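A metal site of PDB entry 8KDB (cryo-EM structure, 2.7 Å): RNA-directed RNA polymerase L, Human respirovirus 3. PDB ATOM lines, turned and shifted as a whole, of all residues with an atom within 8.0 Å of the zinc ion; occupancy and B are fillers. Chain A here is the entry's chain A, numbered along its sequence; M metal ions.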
ATOM      1  N   VAL A 983      -3.167  19.091  19.706  1.00  0.00           N
ATOM      2  CA  VAL A 983      -3.056  17.646  19.601  1.00  0.00           C
ATOM      3  C   VAL A 983      -3.866  16.964  20.697  1.00  0.00           C
ATOM      4  O   VAL A 983      -4.578  15.982  20.456  1.00  0.00           O
ATOM      5  CB  VAL A 983      -1.580  17.213  19.631  1.00  0.00           C
ATOM      6  CG1 VAL A 983      -1.466  15.702  19.617  1.00  0.00           C
ATOM      7  CG2 VAL A 983      -0.841  17.810  18.443  1.00  0.00           C
ATOM      8  N   ALA A 987      -7.085  14.507  20.110  1.00  0.00           N
ATOM      9  CA  ALA A 987      -7.107  13.179  20.714  1.00  0.00           C
ATOM     10  C   ALA A 987      -8.329  13.000  21.605  1.00  0.00           C
ATOM     11  O   ALA A 987      -8.965  11.941  21.602  1.00  0.00           O
ATOM     12  CB  ALA A 987      -5.821  12.944  21.508  1.00  0.00           C
ATOM     13  N   LYS A 990     -11.339  12.430  19.393  1.00  0.00           N
ATOM     14  CA  LYS A 990     -11.377  11.045  18.939  1.00  0.00           C
ATOM     15  C   LYS A 990     -11.880  10.118  20.029  1.00  0.00           C
ATOM     16  O   LYS A 990     -12.698   9.214  19.781  1.00  0.00           O
ATOM     17  CB  LYS A 990     -10.004  10.602  18.450  1.00  0.00           C
ATOM     18  CG  LYS A 990      -9.542  11.289  17.174  1.00  0.00           C
ATOM     19  CD  LYS A 990      -8.151  10.836  16.780  1.00  0.00           C
ATOM     20  CE  LYS A 990      -8.026   9.323  16.820  1.00  0.00           C
ATOM     21  NZ  LYS A 990      -6.601   8.894  16.820  1.00  0.00           N
ATOM     22  N   MET A1156      -7.482   9.003  11.634  1.00  0.00           N
ATOM     23  CA  MET A1156      -6.137   9.553  11.536  1.00  0.00           C
ATOM     24  C   MET A1156      -5.534   9.747  12.929  1.00  0.00           C
ATOM     25  O   MET A1156      -6.223   9.691  13.944  1.00  0.00           O
ATOM     26  CB  MET A1156      -6.166  10.886  10.779  1.00  0.00           C
ATOM     27  CG  MET A1156      -6.193  10.759   9.272  1.00  0.00           C
ATOM     28  SD  MET A1156      -6.969  12.179   8.480  1.00  0.00           S
ATOM     29  CE  MET A1156      -5.577  13.284   8.337  1.00  0.00           C
ATOM     30  N   CYS A1157      -4.224   9.966  12.951  1.00  0.00           N
ATOM     31  CA  CYS A1157      -3.547  10.302  14.197  1.00  0.00           C
ATOM     32  C   CYS A1157      -3.780  11.768  14.531  1.00  0.00           C
ATOM     33  O   CYS A1157      -3.959  12.612  13.646  1.00  0.00           O
ATOM     34  CB  CYS A1157      -2.048  10.017  14.082  1.00  0.00           C
ATOM     35  SG  CYS A1157      -1.129  10.314  15.605  1.00  0.00           S
ATOM     36  N   SER A1158      -3.783  12.077  15.827  1.00  0.00           N
ATOM     37  CA  SER A1158      -4.066  13.437  16.267  1.00  0.00           C
ATOM     38  C   SER A1158      -3.004  14.421  15.801  1.00  0.00           C
ATOM     39  O   SER A1158      -3.305  15.602  15.595  1.00  0.00           O
ATOM     40  CB  SER A1158      -4.216  13.488  17.788  1.00  0.00           C
ATOM     41  OG  SER A1158      -3.101  12.898  18.423  1.00  0.00           O
ATOM     42  N   VAL A1159      -1.757  13.968  15.638  1.00  0.00           N
ATOM     43  CA  VAL A1159      -0.709  14.840  15.118  1.00  0.00           C
ATOM     44  C   VAL A1159      -1.011  15.228  13.672  1.00  0.00           C
ATOM     45  O   VAL A1159      -0.906  16.403  13.294  1.00  0.00           O
ATOM     46  CB  VAL A1159       0.661  14.159  15.238  1.00  0.00           C
ATOM     47  CG1 VAL A1159       1.710  14.901  14.436  1.00  0.00           C
ATOM     48  CG2 VAL A1159       1.074  14.065  16.696  1.00  0.00           C
ATOM     49  N   ASP A1160      -1.412  14.254  12.850  1.00  0.00           N
ATOM     50  CA  ASP A1160      -1.781  14.549  11.478  1.00  0.00           C
ATOM     51  C   ASP A1160      -3.022  15.443  11.421  1.00  0.00           C
ATOM     52  O   ASP A1160      -3.118  16.327  10.560  1.00  0.00           O
ATOM     53  CB  ASP A1160      -2.025  13.252  10.710  1.00  0.00           C
ATOM     54  CG  ASP A1160      -0.744  12.506  10.418  1.00  0.00           C
ATOM     55  OD1 ASP A1160       0.241  13.160  10.022  1.00  0.00           O
ATOM     56  OD2 ASP A1160      -0.724  11.271  10.581  1.00  0.00           O
ATOM     57  N   PRO A1185       3.327  14.559  20.435  1.00  0.00           N
ATOM     58  CA  PRO A1185       2.269  13.607  20.804  1.00  0.00           C
ATOM     59  C   PRO A1185       1.768  13.842  22.219  1.00  0.00           C
ATOM     60  O   PRO A1185       2.469  14.354  23.087  1.00  0.00           O
ATOM     61  CB  PRO A1185       2.952  12.238  20.688  1.00  0.00           C
ATOM     62  CG  PRO A1185       4.289  12.492  20.070  1.00  0.00           C
ATOM     63  CD  PRO A1185       4.645  13.910  20.333  1.00  0.00           C
ATOM     64  N   ASP A1186       0.496  13.451  22.442  1.00  0.00           N
ATOM     65  CA  ASP A1186      -0.025  13.540  23.795  1.00  0.00           C
ATOM     66  C   ASP A1186       0.112  12.201  24.510  1.00  0.00           C
ATOM     67  O   ASP A1186       0.063  11.142  23.875  1.00  0.00           O
ATOM     68  CB  ASP A1186      -1.485  13.976  23.790  1.00  0.00           C
ATOM     69  CG  ASP A1186      -2.386  12.985  23.096  1.00  0.00           C
ATOM     70  OD1 ASP A1186      -1.988  12.494  22.019  1.00  0.00           O
ATOM     71  OD2 ASP A1186      -3.465  12.677  23.640  1.00  0.00           O
ATOM     72  N   GLU A1189      -2.518   8.994  24.201  1.00  0.00           N
ATOM     73  CA  GLU A1189      -2.606   8.299  22.931  1.00  0.00           C
ATOM     74  C   GLU A1189      -1.364   7.472  22.647  1.00  0.00           C
ATOM     75  O   GLU A1189      -1.454   6.388  22.072  1.00  0.00           O
ATOM     76  CB  GLU A1189      -2.849   9.288  21.791  1.00  0.00           C
ATOM     77  CG  GLU A1189      -2.858   8.656  20.413  1.00  0.00           C
ATOM     78  CD  GLU A1189      -3.418   9.569  19.343  1.00  0.00           C
ATOM     79  OE1 GLU A1189      -4.347  10.340  19.645  1.00  0.00           O
ATOM     80  OE2 GLU A1189      -2.921   9.501  18.195  1.00  0.00           O
ATOM     81  N   LEU A1190      -0.188   7.972  23.057  1.00  0.00           N
ATOM     82  CA  LEU A1190       1.067   7.286  22.750  1.00  0.00           C
ATOM     83  C   LEU A1190       1.233   6.020  23.587  1.00  0.00           C
ATOM     84  O   LEU A1190       1.632   4.971  23.060  1.00  0.00           O
ATOM     85  CB  LEU A1190       2.234   8.242  22.982  1.00  0.00           C
ATOM     86  CG  LEU A1190       3.635   7.770  22.576  1.00  0.00           C
ATOM     87  CD1 LEU A1190       3.752   7.673  21.071  1.00  0.00           C
ATOM     88  CD2 LEU A1190       4.684   8.724  23.126  1.00  0.00           C
ATOM     89  N   GLU A1393       3.448   3.725  21.147  1.00  0.00           N
ATOM     90  CA  GLU A1393       2.871   3.431  19.835  1.00  0.00           C
ATOM     91  C   GLU A1393       3.539   4.356  18.817  1.00  0.00           C
ATOM     92  O   GLU A1393       2.998   5.393  18.425  1.00  0.00           O
ATOM     93  CB  GLU A1393       1.359   3.590  19.852  1.00  0.00           C
ATOM     94  CG  GLU A1393       0.642   2.588  20.733  1.00  0.00           C
ATOM     95  CD  GLU A1393      -0.873   2.728  20.653  1.00  0.00           C
ATOM     96  OE1 GLU A1393      -1.349   3.687  20.021  1.00  0.00           O
ATOM     97  OE2 GLU A1393      -1.575   1.879  21.244  1.00  0.00           O
ATOM     98  N   ASP A1394       4.730   3.957  18.384  1.00  0.00           N
ATOM     99  CA  ASP A1394       5.511   4.754  17.448  1.00  0.00           C
ATOM    100  C   ASP A1394       5.039   4.621  16.009  1.00  0.00           C
ATOM    101  O   ASP A1394       5.533   5.358  15.141  1.00  0.00           O
ATOM    102  CB  ASP A1394       6.992   4.368  17.538  1.00  0.00           C
ATOM    103  CG  ASP A1394       7.200   2.881  17.599  1.00  0.00           C
ATOM    104  OD1 ASP A1394       6.203   2.126  17.509  1.00  0.00           O
ATOM    105  OD2 ASP A1394       8.362   2.445  17.733  1.00  0.00           O
ATOM    106  N   GLU A1395       4.099   3.722  15.728  1.00  0.00           N
ATOM    107  CA  GLU A1395       3.635   3.541  14.355  1.00  0.00           C
ATOM    108  C   GLU A1395       2.818   4.740  13.876  1.00  0.00           C
ATOM    109  O   GLU A1395       2.742   4.976  12.663  1.00  0.00           O
ATOM    110  CB  GLU A1395       2.821   2.261  14.246  1.00  0.00           C
ATOM    111  CG  GLU A1395       1.393   2.368  14.766  1.00  0.00           C
ATOM    112  CD  GLU A1395       1.294   2.158  16.261  1.00  0.00           C
ATOM    113  OE1 GLU A1395       2.274   1.645  16.853  1.00  0.00           O
ATOM    114  OE2 GLU A1395       0.253   2.510  16.848  1.00  0.00           O
ATOM    115  N   CYS A1396       2.205   5.495  14.785  1.00  0.00           N
ATOM    116  CA  CYS A1396       1.397   6.634  14.401  1.00  0.00           C
ATOM    117  C   CYS A1396       1.919   7.952  14.957  1.00  0.00           C
ATOM    118  O   CYS A1396       2.143   8.902  14.199  1.00  0.00           O
ATOM    119  CB  CYS A1396      -0.057   6.432  14.840  1.00  0.00           C
ATOM    120  SG  CYS A1396      -0.371   6.674  16.602  1.00  0.00           S
ATOM    121  N   CYS A1397       2.118   8.038  16.272  1.00  0.00           N
ATOM    122  CA  CYS A1397       2.352   9.337  16.904  1.00  0.00           C
ATOM    123  C   CYS A1397       3.763   9.853  16.679  1.00  0.00           C
ATOM    124  O   CYS A1397       3.960  11.051  16.468  1.00  0.00           O
ATOM    125  CB  CYS A1397       2.059   9.246  18.403  1.00  0.00           C
ATOM    126  SG  CYS A1397       0.298   9.245  18.809  1.00  0.00           S
ATOM    127  N   ILE A1398       4.764   8.974  16.712  1.00  0.00           N
ATOM    128  CA  ILE A1398       6.149   9.408  16.581  1.00  0.00           C
ATOM    129  C   ILE A1398       6.460   9.618  15.107  1.00  0.00           C
ATOM    130  O   ILE A1398       6.318   8.704  14.294  1.00  0.00           O
ATOM    131  CB  ILE A1398       7.109   8.380  17.200  1.00  0.00           C
ATOM    132  CG1 ILE A1398       6.893   8.308  18.718  1.00  0.00           C
ATOM    133  CG2 ILE A1398       8.548   8.753  16.893  1.00  0.00           C
ATOM    134  CD1 ILE A1398       7.226   9.595  19.428  1.00  0.00           C
ATOM    135  N   LYS A1399       6.890  10.834  14.768  1.00  0.00           N
ATOM    136  CA  LYS A1399       7.172  11.199  13.389  1.00  0.00           C
ATOM    137  C   LYS A1399       8.590  11.737  13.283  1.00  0.00           C
ATOM    138  O   LYS A1399       8.958  12.691  13.971  1.00  0.00           O
ATOM    139  CB  LYS A1399       6.177  12.249  12.881  1.00  0.00           C
ATOM    140  CG  LYS A1399       4.913  11.659  12.283  1.00  0.00           C
ATOM    141  CD  LYS A1399       3.794  12.675  12.241  1.00  0.00           C
ATOM    142  CE  LYS A1399       2.477  11.994  11.948  1.00  0.00           C
ATOM    143  NZ  LYS A1399       2.325  10.735  12.715  1.00  0.00           N
HETATM  144 ZN    ZN M   1      -1.341   8.708  17.270  1.00  0.00          ZN
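The side-chain carboxylate (OE2) of Glu 1189 is bound to the zinc ion (2.0 Å). SG of Cys 1397 is bound to the zinc ion. SG of Cys 1157 binds the zinc ion. The zinc ion is bound by the side-chain sulfur (SG) of Cys 1396.
Of the 19 residues printed, 4 come within 4 Å of the zinc ion. The nearest printed residue that does not touch the zinc ion is Ser 1158 (4.4 Å).
The side-chain carboxylate of Glu 1189 is in hydrogen-bond range of the side-chain hydroxyl of Ser 1158. The side-chain carboxylate (OE1) of Glu 1189 lies within salt-bridge range of the side-chain amino group (NZ) of Lys 990. The side-chain sulfur of Cys 1157 sits close to the backbone NH of Val 1159 (3.7 Å).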
